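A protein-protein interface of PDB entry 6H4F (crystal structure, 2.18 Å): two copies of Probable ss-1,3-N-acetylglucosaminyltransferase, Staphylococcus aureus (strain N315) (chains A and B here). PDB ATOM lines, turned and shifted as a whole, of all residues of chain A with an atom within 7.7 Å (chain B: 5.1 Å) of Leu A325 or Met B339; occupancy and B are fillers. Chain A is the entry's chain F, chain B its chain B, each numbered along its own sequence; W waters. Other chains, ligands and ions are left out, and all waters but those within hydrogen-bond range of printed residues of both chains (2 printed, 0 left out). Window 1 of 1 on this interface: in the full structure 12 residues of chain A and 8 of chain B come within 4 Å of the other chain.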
ATOM      1  N   LEU A 279      -8.142  30.686   7.838  1.00  0.00           N
ATOM      2  CA  LEU A 279      -9.487  30.435   7.355  1.00  0.00           C
ATOM      3  C   LEU A 279     -10.510  30.657   8.475  1.00  0.00           C
ATOM      4  O   LEU A 279     -11.624  31.045   8.199  1.00  0.00           O
ATOM      5  CB  LEU A 279      -9.572  29.019   6.790  1.00  0.00           C
ATOM      6  CG  LEU A 279      -8.759  28.809   5.511  1.00  0.00           C
ATOM      7  CD1 LEU A 279      -8.741  27.351   5.091  1.00  0.00           C
ATOM      8  CD2 LEU A 279      -9.289  29.694   4.382  1.00  0.00           C
ATOM      9  N   THR A 320      -7.532  21.587   9.175  1.00  0.00           N
ATOM     10  CA  THR A 320      -8.759  20.995   9.679  1.00  0.00           C
ATOM     11  C   THR A 320      -9.720  20.775   8.500  1.00  0.00           C
ATOM     12  O   THR A 320      -9.941  21.691   7.690  1.00  0.00           O
ATOM     13  CB  THR A 320      -9.390  21.868  10.766  1.00  0.00           C
ATOM     14  OG1 THR A 320      -8.383  22.076  11.757  1.00  0.00           O
ATOM     15  CG2 THR A 320     -10.646  21.268  11.369  1.00  0.00           C
ATOM     16  N   GLN A 321     -10.291  19.565   8.416  1.00  0.00           N
ATOM     17  CA  GLN A 321     -10.737  19.036   7.137  1.00  0.00           C
ATOM     18  C   GLN A 321     -12.071  19.624   6.685  1.00  0.00           C
ATOM     19  O   GLN A 321     -12.360  19.538   5.504  1.00  0.00           O
ATOM     20  CB  GLN A 321     -10.699  17.498   7.162  1.00  0.00           C
ATOM     21  CG  GLN A 321      -9.292  16.949   6.914  1.00  0.00           C
ATOM     22  CD  GLN A 321      -8.706  17.356   5.575  1.00  0.00           C
ATOM     23  OE1 GLN A 321      -9.229  16.973   4.527  1.00  0.00           O
ATOM     24  NE2 GLN A 321      -7.621  18.133   5.569  1.00  0.00           N
ATOM     25  N   ILE A 322     -12.837  20.277   7.567  1.00  0.00           N
ATOM     26  CA  ILE A 322     -14.031  21.021   7.122  1.00  0.00           C
ATOM     27  C   ILE A 322     -13.650  22.088   6.090  1.00  0.00           C
ATOM     28  O   ILE A 322     -14.503  22.496   5.325  1.00  0.00           O
ATOM     29  CB  ILE A 322     -14.802  21.673   8.285  1.00  0.00           C
ATOM     30  CG1 ILE A 322     -13.916  22.560   9.154  1.00  0.00           C
ATOM     31  CG2 ILE A 322     -15.539  20.633   9.115  1.00  0.00           C
ATOM     32  CD1 ILE A 322     -14.708  23.489  10.044  1.00  0.00           C
ATOM     33  N   PHE A 323     -12.389  22.540   6.083  1.00  0.00           N
ATOM     34  CA  PHE A 323     -11.932  23.596   5.165  1.00  0.00           C
ATOM     35  C   PHE A 323     -11.310  23.038   3.883  1.00  0.00           C
ATOM     36  O   PHE A 323     -10.784  23.822   3.073  1.00  0.00           O
ATOM     37  CB  PHE A 323     -10.917  24.493   5.877  1.00  0.00           C
ATOM     38  CG  PHE A 323     -11.497  25.275   7.022  1.00  0.00           C
ATOM     39  CD1 PHE A 323     -12.492  26.208   6.797  1.00  0.00           C
ATOM     40  CD2 PHE A 323     -11.092  25.052   8.325  1.00  0.00           C
ATOM     41  CE1 PHE A 323     -13.041  26.938   7.846  1.00  0.00           C
ATOM     42  CE2 PHE A 323     -11.643  25.773   9.369  1.00  0.00           C
ATOM     43  CZ  PHE A 323     -12.620  26.711   9.138  1.00  0.00           C
ATOM     44  N   ASN A 324     -11.395  21.712   3.653  1.00  0.00           N
ATOM     45  CA  ASN A 324     -10.669  21.116   2.527  1.00  0.00           C
ATOM     46  C   ASN A 324     -11.149  21.757   1.204  1.00  0.00           C
ATOM     47  O   ASN A 324     -10.357  22.081   0.344  1.00  0.00           O
ATOM     48  CB  ASN A 324     -10.781  19.583   2.520  1.00  0.00           C
ATOM     49  CG  ASN A 324     -12.117  19.046   2.031  1.00  0.00           C
ATOM     50  OD1 ASN A 324     -13.164  19.526   2.431  1.00  0.00           O
ATOM     51  ND2 ASN A 324     -12.079  18.070   1.132  1.00  0.00           N
ATOM     52  N   LEU A 325     -12.465  21.921   1.048  1.00  0.00           N
ATOM     53  CA  LEU A 325     -13.023  22.433  -0.198  1.00  0.00           C
ATOM     54  C   LEU A 325     -12.683  23.919  -0.354  1.00  0.00           C
ATOM     55  O   LEU A 325     -12.244  24.351  -1.425  1.00  0.00           O
ATOM     56  CB  LEU A 325     -14.532  22.189  -0.216  1.00  0.00           C
ATOM     57  CG  LEU A 325     -15.294  22.891  -1.336  1.00  0.00           C
ATOM     58  CD1 LEU A 325     -14.800  22.423  -2.688  1.00  0.00           C
ATOM     59  CD2 LEU A 325     -16.792  22.660  -1.200  1.00  0.00           C
ATOM     60  N   LYS A 326     -12.862  24.697   0.713  1.00  0.00           N
ATOM     61  CA  LYS A 326     -12.565  26.120   0.628  1.00  0.00           C
ATOM     62  C   LYS A 326     -11.093  26.340   0.250  1.00  0.00           C
ATOM     63  O   LYS A 326     -10.782  27.176  -0.604  1.00  0.00           O
ATOM     64  CB  LYS A 326     -12.893  26.834   1.941  1.00  0.00           C
ATOM     65  CG  LYS A 326     -12.747  28.345   1.823  1.00  0.00           C
ATOM     66  CD  LYS A 326     -13.415  29.120   2.909  1.00  0.00           C
ATOM     67  CE  LYS A 326     -13.343  30.608   2.653  1.00  0.00           C
ATOM     68  NZ  LYS A 326     -14.026  31.350   3.742  1.00  0.00           N
ATOM     69  N   LEU A 327     -10.191  25.581   0.880  1.00  0.00           N
ATOM     70  CA  LEU A 327      -8.761  25.719   0.591  1.00  0.00           C
ATOM     71  C   LEU A 327      -8.480  25.378  -0.880  1.00  0.00           C
ATOM     72  O   LEU A 327      -7.731  26.085  -1.545  1.00  0.00           O
ATOM     73  CB  LEU A 327      -7.976  24.805   1.532  1.00  0.00           C
ATOM     74  CG  LEU A 327      -6.475  24.722   1.296  1.00  0.00           C
ATOM     75  CD1 LEU A 327      -5.852  26.090   1.345  1.00  0.00           C
ATOM     76  CD2 LEU A 327      -5.845  23.794   2.311  1.00  0.00           C
ATOM     77  N   GLU A 328      -9.073  24.293  -1.393  1.00  0.00           N
ATOM     78  CA  GLU A 328      -8.796  23.894  -2.770  1.00  0.00           C
ATOM     79  C   GLU A 328      -9.372  24.955  -3.724  1.00  0.00           C
ATOM     80  O   GLU A 328      -8.746  25.278  -4.734  1.00  0.00           O
ATOM     81  CB  GLU A 328      -9.350  22.498  -3.075  1.00  0.00           C
ATOM     82  CG  GLU A 328      -8.885  21.952  -4.422  1.00  0.00           C
ATOM     83  CD  GLU A 328      -7.374  21.866  -4.585  1.00  0.00           C
ATOM     84  OE1 GLU A 328      -6.709  21.290  -3.680  1.00  0.00           O
ATOM     85  OE2 GLU A 328      -6.861  22.388  -5.605  1.00  0.00           O
ATOM     86  N   ALA A 329     -10.534  25.523  -3.380  1.00  0.00           N
ATOM     87  CA  ALA A 329     -11.152  26.547  -4.210  1.00  0.00           C
ATOM     88  C   ALA A 329     -10.220  27.771  -4.315  1.00  0.00           C
ATOM     89  O   ALA A 329     -10.062  28.362  -5.392  1.00  0.00           O
ATOM     90  CB  ALA A 329     -12.511  26.919  -3.654  1.00  0.00           C
ATOM     91  N   ILE A 330      -9.593  28.141  -3.200  1.00  0.00           N
ATOM     92  CA  ILE A 330      -8.674  29.259  -3.193  1.00  0.00           C
ATOM     93  C   ILE A 330      -7.439  28.924  -4.046  1.00  0.00           C
ATOM     94  O   ILE A 330      -6.985  29.746  -4.829  1.00  0.00           O
ATOM     95  CB  ILE A 330      -8.295  29.667  -1.762  1.00  0.00           C
ATOM     96  CG1 ILE A 330      -9.496  30.241  -1.018  1.00  0.00           C
ATOM     97  CG2 ILE A 330      -7.139  30.651  -1.781  1.00  0.00           C
ATOM     98  CD1 ILE A 330      -9.365  30.217   0.487  1.00  0.00           C
ATOM     99  N   ARG A 331      -6.889  27.718  -3.891  1.00  0.00           N
ATOM    100  CA  ARG A 331      -5.740  27.298  -4.707  1.00  0.00           C
ATOM    101  C   ARG A 331      -6.084  27.367  -6.205  1.00  0.00           C
ATOM    102  O   ARG A 331      -5.237  27.749  -7.003  1.00  0.00           O
ATOM    103  CB  ARG A 331      -5.305  25.874  -4.351  1.00  0.00           C
ATOM    104  CG  ARG A 331      -4.498  25.767  -3.070  1.00  0.00           C
ATOM    105  CD  ARG A 331      -3.781  24.445  -2.978  1.00  0.00           C
ATOM    106  NE  ARG A 331      -3.024  24.286  -1.749  1.00  0.00           N
ATOM    107  CZ  ARG A 331      -1.820  24.798  -1.526  1.00  0.00           C
ATOM    108  NH1 ARG A 331      -1.243  25.536  -2.464  1.00  0.00           N
ATOM    109  NH2 ARG A 331      -1.206  24.557  -0.375  1.00  0.00           N
ATOM    110  N   GLN A 332      -7.324  27.005  -6.569  1.00  0.00           N
ATOM    111  CA  GLN A 332      -7.759  27.008  -7.963  1.00  0.00           C
ATOM    112  C   GLN A 332      -8.150  28.426  -8.418  1.00  0.00           C
ATOM    113  O   GLN A 332      -8.493  28.614  -9.565  1.00  0.00           O
ATOM    114  CB  GLN A 332      -8.966  26.084  -8.156  1.00  0.00           C
ATOM    115  CG  GLN A 332      -8.691  24.618  -7.843  1.00  0.00           C
ATOM    116  CD  GLN A 332      -7.698  24.007  -8.792  1.00  0.00           C
ATOM    117  OE1 GLN A 332      -7.639  24.390  -9.948  1.00  0.00           O
ATOM    118  NE2 GLN A 332      -6.903  23.058  -8.316  1.00  0.00           N
ATOM    119  N   ALA A 337     -16.458  28.621  -6.667  1.00  0.00           N
ATOM    120  CA  ALA A 337     -16.199  27.497  -5.771  1.00  0.00           C
ATOM    121  C   ALA A 337     -15.990  28.006  -4.337  1.00  0.00           C
ATOM    122  O   ALA A 337     -16.398  27.345  -3.379  1.00  0.00           O
ATOM    123  CB  ALA A 337     -15.023  26.701  -6.274  1.00  0.00           C
ATOM    124  N   VAL A 338     -15.368  29.180  -4.179  1.00  0.00           N
ATOM    125  CA  VAL A 338     -15.230  29.756  -2.840  1.00  0.00           C
ATOM    126  C   VAL A 338     -16.615  30.132  -2.295  1.00  0.00           C
ATOM    127  O   VAL A 338     -16.927  29.851  -1.140  1.00  0.00           O
ATOM    128  CB  VAL A 338     -14.270  30.954  -2.793  1.00  0.00           C
ATOM    129  CG1 VAL A 338     -14.148  31.485  -1.370  1.00  0.00           C
ATOM    130  CG2 VAL A 338     -12.894  30.591  -3.321  1.00  0.00           C
ATOM    131  N   ILE A 340     -19.438  28.762  -3.007  1.00  0.00           N
ATOM    132  CA  ILE A 340     -20.122  27.523  -2.700  1.00  0.00           C
ATOM    133  C   ILE A 340     -19.575  26.934  -1.400  1.00  0.00           C
ATOM    134  O   ILE A 340     -20.342  26.501  -0.541  1.00  0.00           O
ATOM    135  CB  ILE A 340     -20.008  26.524  -3.871  1.00  0.00           C
ATOM    136  CG1 ILE A 340     -20.807  27.007  -5.082  1.00  0.00           C
ATOM    137  CG2 ILE A 340     -20.458  25.128  -3.422  1.00  0.00           C
ATOM    138  CD1 ILE A 340     -20.382  26.391  -6.380  1.00  0.00           C
ATOM    139  N   ALA A 341     -18.247  26.929  -1.246  1.00  0.00           N
ATOM    140  CA  ALA A 341     -17.619  26.388  -0.031  1.00  0.00           C
ATOM    141  C   ALA A 341     -18.163  27.107   1.217  1.00  0.00           C
ATOM    142  O   ALA A 341     -18.444  26.467   2.226  1.00  0.00           O
ATOM    143  CB  ALA A 341     -16.122  26.496  -0.113  1.00  0.00           C
ATOM    144  N   ASP A 342     -18.322  28.430   1.129  1.00  0.00           N
ATOM    145  CA  ASP A 342     -18.816  29.231   2.251  1.00  0.00           C
ATOM    146  C   ASP A 342     -20.285  28.913   2.532  1.00  0.00           C
ATOM    147  O   ASP A 342     -20.690  28.881   3.678  1.00  0.00           O
ATOM    148  CB  ASP A 342     -18.585  30.731   2.029  1.00  0.00           C
ATOM    149  CG  ASP A 342     -17.169  31.179   2.386  1.00  0.00           C
ATOM    150  OD1 ASP A 342     -16.478  30.438   3.148  1.00  0.00           O
ATOM    151  OD2 ASP A 342     -16.754  32.258   1.912  1.00  0.00           O
ATOM    152  N   LEU A 344     -21.576  26.019   2.258  1.00  0.00           N
ATOM    153  CA  LEU A 344     -21.614  24.684   2.890  1.00  0.00           C
ATOM    154  C   LEU A 344     -20.992  24.695   4.295  1.00  0.00           C
ATOM    155  O   LEU A 344     -21.184  23.751   5.022  1.00  0.00           O
ATOM    156  CB  LEU A 344     -20.888  23.679   1.994  1.00  0.00           C
ATOM    157  CG  LEU A 344     -21.524  23.443   0.635  1.00  0.00           C
ATOM    158  CD1 LEU A 344     -20.640  22.567  -0.227  1.00  0.00           C
ATOM    159  CD2 LEU A 344     -22.900  22.823   0.793  1.00  0.00           C
ATOM    160  N   LEU A 345     -20.249  25.746   4.654  1.00  0.00           N
ATOM    161  CA  LEU A 345     -19.647  25.876   6.005  1.00  0.00           C
ATOM    162  C   LEU A 345     -20.663  26.485   6.986  1.00  0.00           C
ATOM    163  O   LEU A 345     -21.553  27.274   6.641  1.00  0.00           O
ATOM    164  CB  LEU A 345     -18.395  26.752   5.926  1.00  0.00           C
ATOM    165  CG  LEU A 345     -17.142  26.030   5.419  1.00  0.00           C
ATOM    166  CD1 LEU A 345     -16.069  27.023   5.017  1.00  0.00           C
ATOM    167  CD2 LEU A 345     -16.593  25.036   6.435  1.00  0.00           C
ATOM    168  OXT LEU A 345     -20.617  26.231   8.178  1.00  0.00           O
ATOM    169  N   ALA B 288     -12.243  12.370  -3.945  1.00  0.00           N
ATOM    170  CA  ALA B 288     -12.174  13.798  -4.241  1.00  0.00           C
ATOM    171  C   ALA B 288     -11.885  14.623  -2.975  1.00  0.00           C
ATOM    172  O   ALA B 288     -11.128  15.579  -3.050  1.00  0.00           O
ATOM    173  CB  ALA B 288     -13.451  14.293  -4.906  1.00  0.00           C
ATOM    174  N   ASN B 289     -12.506  14.254  -1.843  1.00  0.00           N
ATOM    175  CA  ASN B 289     -12.327  14.963  -0.583  1.00  0.00           C
ATOM    176  C   ASN B 289     -11.308  14.250   0.329  1.00  0.00           C
ATOM    177  O   ASN B 289     -11.181  14.625   1.482  1.00  0.00           O
ATOM    178  CB  ASN B 289     -13.671  15.123   0.132  1.00  0.00           C
ATOM    179  CG  ASN B 289     -14.521  16.191  -0.494  1.00  0.00           C
ATOM    180  OD1 ASN B 289     -14.133  17.358  -0.535  1.00  0.00           O
ATOM    181  ND2 ASN B 289     -15.712  15.840  -0.936  1.00  0.00           N
ATOM    182  N   LYS B 297      -5.143  12.890  -7.463  1.00  0.00           N
ATOM    183  CA  LYS B 297      -6.573  13.083  -7.626  1.00  0.00           C
ATOM    184  C   LYS B 297      -6.867  13.449  -9.089  1.00  0.00           C
ATOM    185  O   LYS B 297      -7.805  12.939  -9.682  1.00  0.00           O
ATOM    186  CB  LYS B 297      -7.133  14.184  -6.729  1.00  0.00           C
ATOM    187  CG  LYS B 297      -7.219  13.865  -5.257  1.00  0.00           C
ATOM    188  CD  LYS B 297      -7.740  15.055  -4.447  1.00  0.00           C
ATOM    189  CE  LYS B 297      -7.861  14.724  -2.976  1.00  0.00           C
ATOM    190  NZ  LYS B 297      -8.369  15.877  -2.213  1.00  0.00           N
ATOM    191  N   LEU B 335     -12.571  18.684 -10.679  1.00  0.00           N
ATOM    192  CA  LEU B 335     -12.313  18.141  -9.351  1.00  0.00           C
ATOM    193  C   LEU B 335     -13.153  18.872  -8.300  1.00  0.00           C
ATOM    194  O   LEU B 335     -13.751  18.239  -7.430  1.00  0.00           O
ATOM    195  CB  LEU B 335     -10.825  18.236  -9.009  1.00  0.00           C
ATOM    196  CG  LEU B 335     -10.457  17.722  -7.617  1.00  0.00           C
ATOM    197  CD1 LEU B 335     -10.866  16.270  -7.441  1.00  0.00           C
ATOM    198  CD2 LEU B 335      -8.953  17.860  -7.365  1.00  0.00           C
ATOM    199  N   LEU B 336     -13.189  20.208  -8.370  1.00  0.00           N
ATOM    200  CA  LEU B 336     -13.940  20.996  -7.400  1.00  0.00           C
ATOM    201  C   LEU B 336     -15.408  20.555  -7.397  1.00  0.00           C
ATOM    202  O   LEU B 336     -16.022  20.437  -6.330  1.00  0.00           O
ATOM    203  CB  LEU B 336     -13.839  22.483  -7.740  1.00  0.00           C
ATOM    204  CG  LEU B 336     -12.533  23.155  -7.328  1.00  0.00           C
ATOM    205  CD1 LEU B 336     -12.432  24.526  -7.969  1.00  0.00           C
ATOM    206  CD2 LEU B 336     -12.401  23.267  -5.815  1.00  0.00           C
ATOM    207  N   ALA B 337     -15.966  20.320  -8.586  1.00  0.00           N
ATOM    208  CA  ALA B 337     -17.375  19.958  -8.694  1.00  0.00           C
ATOM    209  C   ALA B 337     -17.604  18.550  -8.123  1.00  0.00           C
ATOM    210  O   ALA B 337     -18.649  18.290  -7.513  1.00  0.00           O
ATOM    211  CB  ALA B 337     -17.822  20.063 -10.127  1.00  0.00           C
ATOM    212  N   VAL B 338     -16.635  17.649  -8.294  1.00  0.00           N
ATOM    213  CA  VAL B 338     -16.757  16.316  -7.680  1.00  0.00           C
ATOM    214  C   VAL B 338     -16.707  16.455  -6.150  1.00  0.00           C
ATOM    215  O   VAL B 338     -17.507  15.848  -5.452  1.00  0.00           O
ATOM    216  CB  VAL B 338     -15.703  15.321  -8.188  1.00  0.00           C
ATOM    217  CG1 VAL B 338     -15.880  13.969  -7.529  1.00  0.00           C
ATOM    218  CG2 VAL B 338     -15.729  15.183  -9.696  1.00  0.00           C
ATOM    219  N   MET B 339     -15.788  17.279  -5.642  1.00  0.00           N
ATOM    220  CA  MET B 339     -15.687  17.520  -4.207  1.00  0.00           C
ATOM    221  C   MET B 339     -17.031  18.024  -3.660  1.00  0.00           C
ATOM    222  O   MET B 339     -17.503  17.577  -2.614  1.00  0.00           O
ATOM    223  CB  MET B 339     -14.598  18.556  -3.886  1.00  0.00           C
ATOM    224  CG  MET B 339     -13.208  18.100  -4.210  1.00  0.00           C
ATOM    225  SD  MET B 339     -11.964  19.380  -4.009  1.00  0.00           S
ATOM    226  CE  MET B 339     -11.868  19.491  -2.223  1.00  0.00           C
ATOM    227  N   ILE B 340     -17.628  18.979  -4.373  1.00  0.00           N
ATOM    228  CA  ILE B 340     -18.873  19.596  -3.956  1.00  0.00           C
ATOM    229  C   ILE B 340     -20.002  18.555  -4.000  1.00  0.00           C
ATOM    230  O   ILE B 340     -20.800  18.456  -3.052  1.00  0.00           O
ATOM    231  CB  ILE B 340     -19.196  20.830  -4.809  1.00  0.00           C
ATOM    232  CG1 ILE B 340     -18.198  21.955  -4.533  1.00  0.00           C
ATOM    233  CG2 ILE B 340     -20.624  21.279  -4.557  1.00  0.00           C
ATOM    234  CD1 ILE B 340     -18.121  22.988  -5.637  1.00  0.00           C
ATOM    235  N   ALA B 341     -20.059  17.774  -5.079  1.00  0.00           N
ATOM    236  CA  ALA B 341     -21.095  16.741  -5.211  1.00  0.00           C
ATOM    237  C   ALA B 341     -21.052  15.770  -4.023  1.00  0.00           C
ATOM    238  O   ALA B 341     -22.097  15.386  -3.502  1.00  0.00           O
ATOM    239  CB  ALA B 341     -20.923  15.987  -6.502  1.00  0.00           C
ATOM    240  N   ASP B 342     -19.841  15.383  -3.594  1.00  0.00           N
ATOM    241  CA  ASP B 342     -19.668  14.450  -2.484  1.00  0.00           C
ATOM    242  C   ASP B 342     -20.118  15.095  -1.175  1.00  0.00           C
ATOM    243  O   ASP B 342     -20.696  14.415  -0.340  1.00  0.00           O
ATOM    244  CB  ASP B 342     -18.228  13.929  -2.399  1.00  0.00           C
ATOM    245  CG  ASP B 342     -17.942  12.760  -3.339  1.00  0.00           C
ATOM    246  OD1 ASP B 342     -18.915  12.101  -3.770  1.00  0.00           O
ATOM    247  OD2 ASP B 342     -16.744  12.502  -3.618  1.00  0.00           O
ATOM    248  N   LYS B 343     -19.891  16.400  -1.001  1.00  0.00           N
ATOM    249  CA  LYS B 343     -20.355  17.076   0.202  1.00  0.00           C
ATOM    250  C   LYS B 343     -21.888  17.095   0.262  1.00  0.00           C
ATOM    251  O   LYS B 343     -22.432  17.088   1.346  1.00  0.00           O
ATOM    252  CB  LYS B 343     -19.736  18.473   0.326  1.00  0.00           C
ATOM    253  CG  LYS B 343     -18.267  18.398   0.754  1.00  0.00           C
ATOM    254  CD  LYS B 343     -17.665  19.605   1.361  1.00  0.00           C
ATOM    255  CE  LYS B 343     -16.176  19.404   1.528  1.00  0.00           C
ATOM    256  NZ  LYS B 343     -15.885  18.451   2.617  1.00  0.00           N
HETATM  257  O   HOH W   1      -9.227  17.812   0.177  1.00  0.00           O
HETATM  258  O   HOH W   2     -13.882  17.325   4.866  1.00  0.00           O
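Asn A324 touches Met B339. CA of Leu A325 touches CE of Met B339 (3.8 Å). Leu A325 touches Ile B340. CB of Leu A325 touches CE of Lys B343, 3.7 Å away. Ala A329 touches Leu B336. CG of Gln A332 touches CD1 of Leu B336, 3.7 Å away. Ala A337 touches Leu B336. Ile A340 touches Ile B340.
Water W2 lies within hydrogen-bond range of the backbone carbonyl oxygen (O) of Gln A321 (2.8 Å), the side-chain amino group (NZ) of Lys B343 (3.2 Å) and the side-chain amide oxygen (OD1) of Asn A324 (3.4 Å). Water W1 bridges the side-chain amide nitrogen (ND2) of Asn A324 (3.0 Å) and the side-chain amino group (NZ) of Lys B297 (3.2 Å).
Ile A340 touches its own counterpart, Ile B340. 5 positions are printed for both chains.
The side-chain amide oxygen (OD1) of Asn B289 sits at hydrogen-bond distance from the side-chain amide nitrogen (ND2) of Asn A324 (2.7 Å). The side-chain amide oxygen (OD1) of Asn A324 lies within hydrogen-bond range of the side-chain amino group (NZ) of Lys B343.
ND2 of Asn B289 lies within hydrogen-bond range of O of Met B339, 3.0 Å away. The backbone carbonyl oxygen (O) of Gln A321 sits close to the side-chain amide oxygen (OD1) of Asn A324, at 3.2 Å. The side-chain carboxylate (OE2) of Glu A328 sits at hydrogen-bond distance from the side-chain amide nitrogen (NE2) of Gln A332, at 2.8 Å.
Hydrophobic or aromatic side chains of chain B that line the printed part of chain A: Leu B336, Met B339 and Ile B340. Among the printed residues, no Asp or Glu carboxylate lies within 4 Å of a Lys or Arg side-chain nitrogen of the other chain.
Of the printed residues of chain B, Asn A324 touches Asn B289, Met B339 and Lys B343. Of chain B, only Met B339 (3.8 Å), Ile B340 (3.7 Å) and Lys B343 (3.7 Å) come within 4 Å of Leu A325. Of the printed residues of chain B, Ala A329 touches Leu B336. Printed residues of chain B within 4 Å of Ala A337: Leu B336 (3.8 Å). Leu A345 touches none of the printed residues of chain B. Leu B335 touches none of the printed residues of chain A. Printed residues of chain A within 4 Å of Met B339: Asn A324 and Leu A325. Of the printed residues of chain A, Ile B340 touches Leu A325 and Ile A340. The nearest residue of chain B that does not touch Leu A325 is Leu B336 (4.03 Å). The nearest printed residue of chain A that does not touch Met B339 is Glu A328 (4.01 Å). The nearest printed residue of chain B that does not touch Ala A329 is Met B339 (6.3 Å).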
